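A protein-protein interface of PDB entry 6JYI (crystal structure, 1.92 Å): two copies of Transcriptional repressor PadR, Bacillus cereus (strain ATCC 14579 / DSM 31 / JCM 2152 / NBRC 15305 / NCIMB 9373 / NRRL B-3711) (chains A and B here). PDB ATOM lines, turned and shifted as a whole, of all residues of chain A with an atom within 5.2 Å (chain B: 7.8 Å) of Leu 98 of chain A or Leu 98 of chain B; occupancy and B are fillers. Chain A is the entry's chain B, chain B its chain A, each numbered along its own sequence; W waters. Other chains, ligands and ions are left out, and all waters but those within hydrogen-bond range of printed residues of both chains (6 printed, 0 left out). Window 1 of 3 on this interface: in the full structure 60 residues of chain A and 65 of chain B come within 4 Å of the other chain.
O of Phe 35 of chain B is in hydrogen-bond range of N of Asp 40 of chain B (3.3 Å).
A ring nitrogen (ND1) of His 37 of chain B is in hydrogen-bond range of the side-chain hydroxyl (OH) of Tyr 161 of chain B (2.8 Å).
The backbone NH (N) of Leu 103 of chain B lies within hydrogen-bond range of the side-chain hydroxyl (OG) of Ser 100 of chain B.
The side-chain amino group (NZ) of Lys 128 of chain B lies within hydrogen-bond range of the side-chain amide oxygen (OE1) of Gln 164 of chain B, at 2.8 Å.
OG of Ser 100 of chain A lies within hydrogen-bond range of N of Leu 103 of chain A (3.3 Å).
Of the 10 printed residues of chain A, 10 touch a printed residue of chain B.
Hydrophobic or aromatic side chains of chain A within 4 Å of the printed part of chain B: Phe 38, Val 97, Leu 98 and Leu 103.
Of the 20 printed residues of chain B, 12 touch a printed residue of chain A.
Among the printed residues, 32 pairs touch across the chains.
Among the printed residues, Asp or Glu carboxylates within 4 Å of a Lys or Arg side-chain nitrogen of the other chain: Asp 40 of chain A with Arg 99 of chain B (2.8 Å) and Asp 96 of chain A with Lys 128 of chain B (3.1 Å).
Leu 98 of chain B touches His 37 of chain A.
Arg 99 of chain B touches Phe 38 of chain A.
Phe 38 of chain A touches Leu 103 of chain B.
Val 97 of chain B touches Asp 40 of chain A.
Asp 40 of chain A touches Leu 98 of chain B.
Val 97 of chain A touches Asp 40 of chain B (CG1 to O, 3.7 Å).
Leu 98 of chain A touches Phe 38 of chain B (O to C, 3.3 Å).
Leu 98 of chain A touches Val 97 of chain B (CA to O, 3.6 Å).
Arg 99 of chain A touches Phe 38 of chain B (CA to O, 3.4 Å).
Leu 103 of chain A touches Phe 38 of chain B.
Asp 40 of chain A touches Arg 99 of chain B, and with the chains exchanged Arg 99 of chain A touches Asp 40 of chain B.
Asp 96 of chain A touches Asp 40 of chain B, but with the chains exchanged Asp 40 of chain A does not touch Asp 96 of chain B (7.8 Å).
Asp 96 of chain A touches Ser 100 of chain B, and with the chains exchanged Ser 100 of chain A touches Asp 96 of chain B.
Val 97 of chain A touches Arg 99 of chain B, and with the chains exchanged Arg 99 of chain A touches Val 97 of chain B.
Positions printed for both chains: 37, 38, 39, 40, 96, 97, 98, 99, 100 and 103.
Of the printed residues of chain B, His 37 of chain A touches Leu 98 (3.5 Å).
Of the printed residues of chain B, Val 97 of chain A touches Asp 40, Gly 41, Val 97, Leu 98 and Arg 99.
Leu 98 of chain A touches just these residues of chain B: His 37, Phe 38, Phe 39, Asp 40, Val 97 and Leu 98.
Of the printed residues of chain A, Gly 41 of chain B touches Val 97 (3.9 Å).
Of chain A, only His 37, Phe 38, Phe 39, Asp 40, Val 97 and Leu 98 come within 4 Å of Leu 98 of chain B.
Water W6 bridges OD1 of Asp 96 of chain A and N of Asp 101 of chain B.
Water W4 bridges O of Val 97 of chain A (2.7 Å) and O of Val 97 of chain B (2.9 Å).
Water W5 lies within hydrogen-bond range of O of Lys 95 of chain B (2.8 Å) and O of Arg 99 of chain A (2.9 Å).
Water W1 lies within hydrogen-bond range of the backbone NH of Leu 98 of chain B (2.8 Å) and the backbone carbonyl oxygen of Phe 39 of chain A (3.5 Å).
Water W3 lies within hydrogen-bond range of O of Thr 36 of chain B, N of Leu 98 of chain A and O of Asp 96 of chain A.
Water W2 lies within hydrogen-bond range of the backbone carbonyl oxygen (O) of Phe 38 of chain A and the backbone carbonyl oxygen (O) of Ser 100 of chain B.
The backbone carbonyl oxygen (O) of Phe 38 of chain B sits at hydrogen-bond distance from the backbone NH (N) of Ser 100 of chain A (2.7 Å).
The backbone NH (N) of Phe 39 of chain B sits at hydrogen-bond distance from the backbone carbonyl oxygen (O) of Leu 98 of chain A, at 3.4 Å.
The backbone carbonyl oxygen (O) of Leu 98 of chain A is in hydrogen-bond range of the backbone NH (N) of Asp 40 of chain B (3.0 Å).
OD1 of Asp 96 of chain B sits at hydrogen-bond distance from OG of Ser 100 of chain A (2.8 Å).
O of Arg 99 of chain A lies within hydrogen-bond range of N of Val 97 of chain B, 2.9 Å away.
N of Phe 39 of chain A lies within hydrogen-bond range of O of Leu 98 of chain B (3.2 Å).
The guanidinium group (NH1) of Arg 99 of chain B lies within salt-bridge range of the side-chain carboxylate (OD2) of Asp 40 of chain A (2.8 Å).
The backbone NH (N) of Arg 99 of chain B is in hydrogen-bond range of the backbone carbonyl oxygen (O) of Val 97 of chain A (2.9 Å).
The backbone carbonyl oxygen (O) of Phe 38 of chain A sits at hydrogen-bond distance from the backbone NH (N) of Ser 100 of chain B (2.8 Å).
OD1 of Asp 96 of chain A sits at hydrogen-bond distance from OG of Ser 100 of chain B, at 2.8 Å.
NZ of Lys 128 of chain B is in salt-bridge range of OD2 of Asp 96 of chain A, at 3.1 Å.
O of Phe 38 of chain A sits close to O of Leu 98 of chain B, 3.3 Å away.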
ATOM      1  N   HIS A  37      36.537  20.660 -23.505  1.00  0.00           N
ATOM      2  CA  HIS A  37      35.375  20.007 -24.098  1.00  0.00           C
ATOM      3  C   HIS A  37      34.021  20.594 -23.637  1.00  0.00           C
ATOM      4  O   HIS A  37      32.996  20.397 -24.300  1.00  0.00           O
ATOM      5  CB  HIS A  37      35.423  18.508 -23.788  1.00  0.00           C
ATOM      6  CG  HIS A  37      36.443  17.769 -24.595  1.00  0.00           C
ATOM      7  ND1 HIS A  37      36.307  17.575 -25.948  1.00  0.00           N
ATOM      8  CD2 HIS A  37      37.628  17.206 -24.249  1.00  0.00           C
ATOM      9  CE1 HIS A  37      37.360  16.922 -26.407  1.00  0.00           C
ATOM     10  NE2 HIS A  37      38.166  16.668 -25.391  1.00  0.00           N
ATOM     11  N   PHE A  38      33.992  21.307 -22.529  1.00  0.00           N
ATOM     12  CA  PHE A  38      32.712  21.873 -22.062  1.00  0.00           C
ATOM     13  C   PHE A  38      32.764  23.238 -21.393  1.00  0.00           C
ATOM     14  O   PHE A  38      31.764  23.703 -20.875  1.00  0.00           O
ATOM     15  CB  PHE A  38      31.958  20.869 -21.230  1.00  0.00           C
ATOM     16  CG  PHE A  38      32.674  20.408 -19.992  1.00  0.00           C
ATOM     17  CD1 PHE A  38      32.576  21.118 -18.822  1.00  0.00           C
ATOM     18  CD2 PHE A  38      33.388  19.216 -19.994  1.00  0.00           C
ATOM     19  CE1 PHE A  38      33.214  20.644 -17.650  1.00  0.00           C
ATOM     20  CE2 PHE A  38      34.007  18.744 -18.838  1.00  0.00           C
ATOM     21  CZ  PHE A  38      33.918  19.447 -17.686  1.00  0.00           C
ATOM     22  N   PHE A  39      33.894  23.927 -21.513  1.00  0.00           N
ATOM     23  CA  PHE A  39      33.975  25.317 -21.056  1.00  0.00           C
ATOM     24  C   PHE A  39      34.579  26.160 -22.180  1.00  0.00           C
ATOM     25  O   PHE A  39      35.503  25.731 -22.833  1.00  0.00           O
ATOM     26  CB  PHE A  39      34.748  25.433 -19.720  1.00  0.00           C
ATOM     27  CG  PHE A  39      34.705  26.806 -19.125  1.00  0.00           C
ATOM     28  CD1 PHE A  39      33.505  27.369 -18.711  1.00  0.00           C
ATOM     29  CD2 PHE A  39      35.845  27.556 -19.012  1.00  0.00           C
ATOM     30  CE1 PHE A  39      33.450  28.663 -18.212  1.00  0.00           C
ATOM     31  CE2 PHE A  39      35.787  28.870 -18.501  1.00  0.00           C
ATOM     32  CZ  PHE A  39      34.613  29.397 -18.103  1.00  0.00           C
ATOM     33  N   ASP A  40      34.033  27.358 -22.404  1.00  0.00           N
ATOM     34  CA  ASP A  40      34.441  28.212 -23.504  1.00  0.00           C
ATOM     35  C   ASP A  40      35.538  29.232 -23.171  1.00  0.00           C
ATOM     36  O   ASP A  40      36.018  29.914 -24.058  1.00  0.00           O
ATOM     37  CB  ASP A  40      33.214  28.948 -24.099  1.00  0.00           C
ATOM     38  CG  ASP A  40      32.460  29.807 -23.082  1.00  0.00           C
ATOM     39  OD1 ASP A  40      32.498  29.555 -21.870  1.00  0.00           O
ATOM     40  OD2 ASP A  40      31.776  30.746 -23.508  1.00  0.00           O
ATOM     41  N   ASP A  96      22.965  24.675 -22.039  1.00  0.00           N
ATOM     42  CA  ASP A  96      24.158  24.521 -22.845  1.00  0.00           C
ATOM     43  C   ASP A  96      24.236  25.599 -23.926  1.00  0.00           C
ATOM     44  O   ASP A  96      23.205  25.947 -24.504  1.00  0.00           O
ATOM     45  CB  ASP A  96      24.139  23.172 -23.572  1.00  0.00           C
ATOM     46  CG  ASP A  96      24.654  22.036 -22.751  1.00  0.00           C
ATOM     47  OD1 ASP A  96      24.991  22.180 -21.552  1.00  0.00           O
ATOM     48  OD2 ASP A  96      24.740  20.951 -23.349  1.00  0.00           O
ATOM     49  N   VAL A  97      25.449  26.085 -24.221  1.00  0.00           N
ATOM     50  CA  VAL A  97      25.677  27.005 -25.327  1.00  0.00           C
ATOM     51  C   VAL A  97      26.728  26.403 -26.259  1.00  0.00           C
ATOM     52  O   VAL A  97      27.902  26.327 -25.924  1.00  0.00           O
ATOM     53  CB  VAL A  97      26.176  28.395 -24.870  1.00  0.00           C
ATOM     54  CG1 VAL A  97      26.270  29.343 -26.091  1.00  0.00           C
ATOM     55  CG2 VAL A  97      25.275  28.970 -23.787  1.00  0.00           C
ATOM     56  N   LEU A  98      26.269  25.945 -27.413  1.00  0.00           N
ATOM     57  CA  LEU A  98      27.115  25.342 -28.418  1.00  0.00           C
ATOM     58  C   LEU A  98      27.224  26.191 -29.685  1.00  0.00           C
ATOM     59  O   LEU A  98      26.205  26.636 -30.230  1.00  0.00           O
ATOM     60  CB  LEU A  98      26.549  23.976 -28.824  1.00  0.00           C
ATOM     61  CG  LEU A  98      27.274  23.291 -29.997  1.00  0.00           C
ATOM     62  CD1 LEU A  98      28.708  23.007 -29.593  1.00  0.00           C
ATOM     63  CD2 LEU A  98      26.545  21.953 -30.373  1.00  0.00           C
ATOM     64  N   ARG A  99      28.453  26.391 -30.141  1.00  0.00           N
ATOM     65  CA  ARG A  99      28.718  26.946 -31.464  1.00  0.00           C
ATOM     66  C   ARG A  99      29.547  25.943 -32.261  1.00  0.00           C
ATOM     67  O   ARG A  99      30.671  25.614 -31.888  1.00  0.00           O
ATOM     68  CB  ARG A  99      29.441  28.286 -31.361  1.00  0.00           C
ATOM     69  CG  ARG A  99      28.899  29.223 -30.286  1.00  0.00           C
ATOM     70  CD  ARG A  99      29.425  30.663 -30.537  1.00  0.00           C
ATOM     71  NE  ARG A  99      30.775  30.613 -31.112  1.00  0.00           N
ATOM     72  CZ  ARG A  99      31.888  30.939 -30.451  1.00  0.00           C
ATOM     73  NH1 ARG A  99      31.816  31.369 -29.198  1.00  0.00           N
ATOM     74  NH2 ARG A  99      33.068  30.844 -31.048  1.00  0.00           N
ATOM     75  N   SER A 100      28.971  25.439 -33.340  1.00  0.00           N
ATOM     76  CA  SER A 100      29.586  24.446 -34.174  1.00  0.00           C
ATOM     77  C   SER A 100      29.597  24.987 -35.613  1.00  0.00           C
ATOM     78  O   SER A 100      28.554  25.001 -36.303  1.00  0.00           O
ATOM     79  CB  SER A 100      28.801  23.131 -34.116  1.00  0.00           C
ATOM     80  OG  SER A 100      29.351  22.164 -35.025  1.00  0.00           O
ATOM     81  N   LEU A 103      28.443  22.294 -38.204  1.00  0.00           N
ATOM     82  CA  LEU A 103      27.026  22.085 -38.422  1.00  0.00           C
ATOM     83  C   LEU A 103      26.434  23.239 -39.221  1.00  0.00           C
ATOM     84  O   LEU A 103      25.494  23.051 -39.988  1.00  0.00           O
ATOM     85  CB  LEU A 103      26.274  21.854 -37.115  1.00  0.00           C
ATOM     86  CG  LEU A 103      26.595  20.496 -36.434  1.00  0.00           C
ATOM     87  CD1 LEU A 103      25.976  20.327 -35.033  1.00  0.00           C
ATOM     88  CD2 LEU A 103      26.254  19.294 -37.350  1.00  0.00           C
ATOM     89  N   PHE B  35      19.085  27.582 -34.747  1.00  0.00           N
ATOM     90  CA  PHE B  35      20.480  27.948 -34.411  1.00  0.00           C
ATOM     91  C   PHE B  35      20.844  27.903 -32.921  1.00  0.00           C
ATOM     92  O   PHE B  35      22.017  27.794 -32.578  1.00  0.00           O
ATOM     93  CB  PHE B  35      20.877  29.294 -35.043  1.00  0.00           C
ATOM     94  CG  PHE B  35      20.988  29.248 -36.520  1.00  0.00           C
ATOM     95  CD1 PHE B  35      19.902  29.431 -37.323  1.00  0.00           C
ATOM     96  CD2 PHE B  35      22.177  28.994 -37.132  1.00  0.00           C
ATOM     97  CE1 PHE B  35      20.015  29.390 -38.719  1.00  0.00           C
ATOM     98  CE2 PHE B  35      22.247  28.947 -38.517  1.00  0.00           C
ATOM     99  CZ  PHE B  35      21.157  29.147 -39.285  1.00  0.00           C
ATOM    100  N   THR B  36      19.866  27.964 -32.028  1.00  0.00           N
ATOM    101  CA  THR B  36      20.107  27.728 -30.592  1.00  0.00           C
ATOM    102  C   THR B  36      20.804  26.349 -30.365  1.00  0.00           C
ATOM    103  O   THR B  36      21.454  26.133 -29.337  1.00  0.00           O
ATOM    104  CB  THR B  36      18.776  27.842 -29.794  1.00  0.00           C
ATOM    105  OG1 THR B  36      18.985  27.725 -28.367  1.00  0.00           O
ATOM    106  CG2 THR B  36      17.843  26.782 -30.212  1.00  0.00           C
ATOM    107  N   HIS B  37      20.669  25.428 -31.317  1.00  0.00           N
ATOM    108  CA  HIS B  37      21.212  24.091 -31.139  1.00  0.00           C
ATOM    109  C   HIS B  37      22.640  23.948 -31.635  1.00  0.00           C
ATOM    110  O   HIS B  37      23.366  23.055 -31.175  1.00  0.00           O
ATOM    111  CB  HIS B  37      20.300  23.041 -31.776  1.00  0.00           C
ATOM    112  CG  HIS B  37      18.951  22.975 -31.134  1.00  0.00           C
ATOM    113  ND1 HIS B  37      18.746  22.431 -29.881  1.00  0.00           N
ATOM    114  CD2 HIS B  37      17.742  23.411 -31.558  1.00  0.00           C
ATOM    115  CE1 HIS B  37      17.466  22.526 -29.565  1.00  0.00           C
ATOM    116  NE2 HIS B  37      16.832  23.112 -30.567  1.00  0.00           N
ATOM    117  N   PHE B  38      23.064  24.811 -32.560  1.00  0.00           N
ATOM    118  CA  PHE B  38      24.416  24.682 -33.081  1.00  0.00           C
ATOM    119  C   PHE B  38      25.189  25.983 -33.334  1.00  0.00           C
ATOM    120  O   PHE B  38      26.362  25.919 -33.688  1.00  0.00           O
ATOM    121  CB  PHE B  38      24.429  23.748 -34.303  1.00  0.00           C
ATOM    122  CG  PHE B  38      23.730  24.298 -35.505  1.00  0.00           C
ATOM    123  CD1 PHE B  38      24.357  25.232 -36.305  1.00  0.00           C
ATOM    124  CD2 PHE B  38      22.452  23.834 -35.858  1.00  0.00           C
ATOM    125  CE1 PHE B  38      23.719  25.762 -37.415  1.00  0.00           C
ATOM    126  CE2 PHE B  38      21.816  24.339 -36.994  1.00  0.00           C
ATOM    127  CZ  PHE B  38      22.435  25.307 -37.751  1.00  0.00           C
ATOM    128  N   PHE B  39      24.562  27.152 -33.129  1.00  0.00           N
ATOM    129  CA  PHE B  39      25.284  28.415 -33.153  1.00  0.00           C
ATOM    130  C   PHE B  39      24.585  29.402 -32.218  1.00  0.00           C
ATOM    131  O   PHE B  39      24.025  30.424 -32.638  1.00  0.00           O
ATOM    132  CB  PHE B  39      25.474  28.970 -34.586  1.00  0.00           C
ATOM    133  CG  PHE B  39      26.862  29.538 -34.844  1.00  0.00           C
ATOM    134  CD1 PHE B  39      27.905  28.702 -35.321  1.00  0.00           C
ATOM    135  CD2 PHE B  39      27.139  30.871 -34.570  1.00  0.00           C
ATOM    136  CE1 PHE B  39      29.191  29.202 -35.532  1.00  0.00           C
ATOM    137  CE2 PHE B  39      28.405  31.382 -34.784  1.00  0.00           C
ATOM    138  CZ  PHE B  39      29.446  30.540 -35.270  1.00  0.00           C
ATOM    139  N   ASP B  40      24.631  29.053 -30.937  1.00  0.00           N
ATOM    140  CA  ASP B  40      23.971  29.773 -29.878  1.00  0.00           C
ATOM    141  C   ASP B  40      24.924  30.793 -29.291  1.00  0.00           C
ATOM    142  O   ASP B  40      26.144  30.714 -29.481  1.00  0.00           O
ATOM    143  CB  ASP B  40      23.538  28.777 -28.788  1.00  0.00           C
ATOM    144  CG  ASP B  40      22.510  29.351 -27.813  1.00  0.00           C
ATOM    145  OD1 ASP B  40      21.727  30.278 -28.198  1.00  0.00           O
ATOM    146  OD2 ASP B  40      22.503  28.863 -26.668  1.00  0.00           O
ATOM    147  N   GLY B  41      24.348  31.743 -28.565  1.00  0.00           N
ATOM    148  CA  GLY B  41      25.110  32.755 -27.838  1.00  0.00           C
ATOM    149  C   GLY B  41      24.862  34.158 -28.353  1.00  0.00           C
ATOM    150  O   GLY B  41      25.182  35.132 -27.679  1.00  0.00           O
ATOM    151  N   LYS B  95      36.824  24.602 -34.866  1.00  0.00           N
ATOM    152  CA  LYS B  95      36.426  23.621 -33.848  1.00  0.00           C
ATOM    153  C   LYS B  95      35.180  24.041 -33.076  1.00  0.00           C
ATOM    154  O   LYS B  95      34.881  25.246 -32.947  1.00  0.00           O
ATOM    155  CB  LYS B  95      37.607  23.351 -32.873  1.00  0.00           C
ATOM    156  CG  LYS B  95      37.850  24.479 -31.830  1.00  0.00           C
ATOM    157  CD  LYS B  95      38.863  24.161 -30.744  1.00  0.00           C
ATOM    158  CE  LYS B  95      38.223  23.734 -29.361  1.00  0.00           C
ATOM    159  NZ  LYS B  95      37.121  24.641 -28.753  1.00  0.00           N
ATOM    160  N   ASP B  96      34.415  23.052 -32.600  1.00  0.00           N
ATOM    161  CA  ASP B  96      33.248  23.301 -31.780  1.00  0.00           C
ATOM    162  C   ASP B  96      33.676  24.056 -30.532  1.00  0.00           C
ATOM    163  O   ASP B  96      34.758  23.808 -29.990  1.00  0.00           O
ATOM    164  CB  ASP B  96      32.608  21.998 -31.310  1.00  0.00           C
ATOM    165  CG  ASP B  96      31.879  21.250 -32.430  1.00  0.00           C
ATOM    166  OD1 ASP B  96      31.758  21.779 -33.555  1.00  0.00           O
ATOM    167  OD2 ASP B  96      31.408  20.127 -32.160  1.00  0.00           O
ATOM    168  N   VAL B  97      32.820  24.964 -30.068  1.00  0.00           N
ATOM    169  CA  VAL B  97      33.026  25.615 -28.783  1.00  0.00           C
ATOM    170  C   VAL B  97      31.756  25.369 -27.966  1.00  0.00           C
ATOM    171  O   VAL B  97      30.679  25.838 -28.344  1.00  0.00           O
ATOM    172  CB  VAL B  97      33.257  27.121 -28.962  1.00  0.00           C
ATOM    173  CG1 VAL B  97      33.351  27.873 -27.598  1.00  0.00           C
ATOM    174  CG2 VAL B  97      34.485  27.406 -29.868  1.00  0.00           C
ATOM    175  N   LEU B  98      31.898  24.727 -26.801  1.00  0.00           N
ATOM    176  CA  LEU B  98      30.754  24.409 -25.924  1.00  0.00           C
ATOM    177  C   LEU B  98      30.939  24.932 -24.525  1.00  0.00           C
ATOM    178  O   LEU B  98      32.010  24.773 -23.941  1.00  0.00           O
ATOM    179  CB  LEU B  98      30.513  22.893 -25.867  1.00  0.00           C
ATOM    180  CG  LEU B  98      29.430  22.396 -24.900  1.00  0.00           C
ATOM    181  CD1 LEU B  98      27.989  22.719 -25.357  1.00  0.00           C
ATOM    182  CD2 LEU B  98      29.571  20.888 -24.672  1.00  0.00           C
ATOM    183  N   ARG B  99      29.892  25.579 -23.992  1.00  0.00           N
ATOM    184  CA  ARG B  99      29.840  25.936 -22.571  1.00  0.00           C
ATOM    185  C   ARG B  99      28.694  25.172 -21.977  1.00  0.00           C
ATOM    186  O   ARG B  99      27.542  25.513 -22.232  1.00  0.00           O
ATOM    187  CB  ARG B  99      29.630  27.438 -22.342  1.00  0.00           C
ATOM    188  CG  ARG B  99      29.553  27.814 -20.853  1.00  0.00           C
ATOM    189  CD  ARG B  99      29.662  29.301 -20.565  1.00  0.00           C
ATOM    190  NE  ARG B  99      28.418  30.027 -20.818  1.00  0.00           N
ATOM    191  CZ  ARG B  99      28.189  30.857 -21.848  1.00  0.00           C
ATOM    192  NH1 ARG B  99      29.114  31.096 -22.785  1.00  0.00           N
ATOM    193  NH2 ARG B  99      26.999  31.458 -21.958  1.00  0.00           N
ATOM    194  N   SER B 100      28.998  24.139 -21.186  1.00  0.00           N
ATOM    195  CA  SER B 100      27.984  23.382 -20.478  1.00  0.00           C
ATOM    196  C   SER B 100      28.166  23.543 -18.973  1.00  0.00           C
ATOM    197  O   SER B 100      29.014  22.873 -18.367  1.00  0.00           O
ATOM    198  CB  SER B 100      28.076  21.901 -20.842  1.00  0.00           C
ATOM    199  OG  SER B 100      27.113  21.150 -20.129  1.00  0.00           O
ATOM    200  N   ASP B 101      27.358  24.420 -18.390  1.00  0.00           N
ATOM    201  CA  ASP B 101      27.253  24.609 -16.945  1.00  0.00           C
ATOM    202  C   ASP B 101      26.926  23.275 -16.251  1.00  0.00           C
ATOM    203  O   ASP B 101      27.503  22.956 -15.206  1.00  0.00           O
ATOM    204  CB  ASP B 101      26.166  25.648 -16.674  1.00  0.00           C
ATOM    205  CG  ASP B 101      26.112  26.114 -15.243  1.00  0.00           C
ATOM    206  OD1 ASP B 101      27.074  25.950 -14.473  1.00  0.00           O
ATOM    207  OD2 ASP B 101      25.070  26.669 -14.886  1.00  0.00           O
ATOM    208  N   LEU B 103      27.720  20.093 -17.202  1.00  0.00           N
ATOM    209  CA  LEU B 103      28.875  19.221 -17.081  1.00  0.00           C
ATOM    210  C   LEU B 103      29.876  19.724 -16.026  1.00  0.00           C
ATOM    211  O   LEU B 103      30.542  18.909 -15.392  1.00  0.00           O
ATOM    212  CB  LEU B 103      29.548  18.959 -18.420  1.00  0.00           C
ATOM    213  CG  LEU B 103      28.692  18.145 -19.408  1.00  0.00           C
ATOM    214  CD1 LEU B 103      29.350  18.035 -20.794  1.00  0.00           C
ATOM    215  CD2 LEU B 103      28.392  16.769 -18.838  1.00  0.00           C
ATOM    216  N   LYS B 128      17.009  17.737 -22.898  1.00  0.00           N
ATOM    217  CA  LYS B 128      17.504  17.180 -24.164  1.00  0.00           C
ATOM    218  C   LYS B 128      16.404  16.422 -24.906  1.00  0.00           C
ATOM    219  O   LYS B 128      16.320  16.501 -26.136  1.00  0.00           O
ATOM    220  CB  LYS B 128      18.764  16.317 -23.960  1.00  0.00           C
ATOM    221  CG  LYS B 128      20.008  17.112 -23.441  1.00  0.00           C
ATOM    222  CD  LYS B 128      20.802  17.697 -24.568  1.00  0.00           C
ATOM    223  CE  LYS B 128      21.700  18.888 -24.163  1.00  0.00           C
ATOM    224  NZ  LYS B 128      22.813  18.530 -23.245  1.00  0.00           N
ATOM    225  N   GLY B 157      22.753  16.520 -34.730  1.00  0.00           N
ATOM    226  CA  GLY B 157      22.240  17.056 -33.487  1.00  0.00           C
ATOM    227  C   GLY B 157      21.412  16.097 -32.701  1.00  0.00           C
ATOM    228  O   GLY B 157      21.651  15.912 -31.501  1.00  0.00           O
ATOM    229  N   SER B 160      23.605  13.221 -31.328  1.00  0.00           N
ATOM    230  CA  SER B 160      24.361  13.643 -30.180  1.00  0.00           C
ATOM    231  C   SER B 160      23.499  13.806 -28.924  1.00  0.00           C
ATOM    232  O   SER B 160      23.798  13.242 -27.884  1.00  0.00           O
ATOM    233  CB  SER B 160      25.099  14.936 -30.539  1.00  0.00           C
ATOM    234  OG  SER B 160      25.629  15.511 -29.373  1.00  0.00           O
ATOM    235  N   TYR B 161      22.394  14.528 -29.030  1.00  0.00           N
ATOM    236  CA  TYR B 161      21.456  14.636 -27.928  1.00  0.00           C
ATOM    237  C   TYR B 161      20.933  13.304 -27.419  1.00  0.00           C
ATOM    238  O   TYR B 161      20.768  13.114 -26.197  1.00  0.00           O
ATOM    239  CB  TYR B 161      20.253  15.482 -28.318  1.00  0.00           C
ATOM    240  CG  TYR B 161      20.482  16.973 -28.438  1.00  0.00           C
ATOM    241  CD1 TYR B 161      21.410  17.635 -27.657  1.00  0.00           C
ATOM    242  CD2 TYR B 161      19.694  17.732 -29.295  1.00  0.00           C
ATOM    243  CE1 TYR B 161      21.585  19.017 -27.766  1.00  0.00           C
ATOM    244  CE2 TYR B 161      19.846  19.076 -29.406  1.00  0.00           C
ATOM    245  CZ  TYR B 161      20.786  19.729 -28.645  1.00  0.00           C
ATOM    246  OH  TYR B 161      20.904  21.095 -28.773  1.00  0.00           O
ATOM    247  N   GLN B 164      23.603  11.586 -25.458  1.00  0.00           N
ATOM    248  CA  GLN B 164      23.689  12.240 -24.128  1.00  0.00           C
ATOM    249  C   GLN B 164      22.577  11.777 -23.194  1.00  0.00           C
ATOM    250  O   GLN B 164      22.842  11.450 -22.056  1.00  0.00           O
ATOM    251  CB  GLN B 164      23.626  13.752 -24.247  1.00  0.00           C
ATOM    252  CG  GLN B 164      24.867  14.343 -24.900  1.00  0.00           C
ATOM    253  CD  GLN B 164      24.646  15.754 -25.355  1.00  0.00           C
ATOM    254  OE1 GLN B 164      23.854  16.479 -24.756  1.00  0.00           O
ATOM    255  NE2 GLN B 164      25.298  16.150 -26.438  1.00  0.00           N
HETATM  256  O   HOH W   1      34.359  24.105 -25.659  1.00  0.00           O
HETATM  257  O   HOH W   2      31.172  24.881 -18.346  1.00  0.00           O
HETATM  258  O   HOH W   3      23.371  25.301 -27.496  1.00  0.00           O
HETATM  259  O   HOH W   4      29.678  28.076 -26.833  1.00  0.00           O
HETATM  260  O   HOH W   5      32.577  26.340 -33.994  1.00  0.00           O
HETATM  261  O   HOH W   6      24.314  23.143 -19.256  1.00  0.00           O
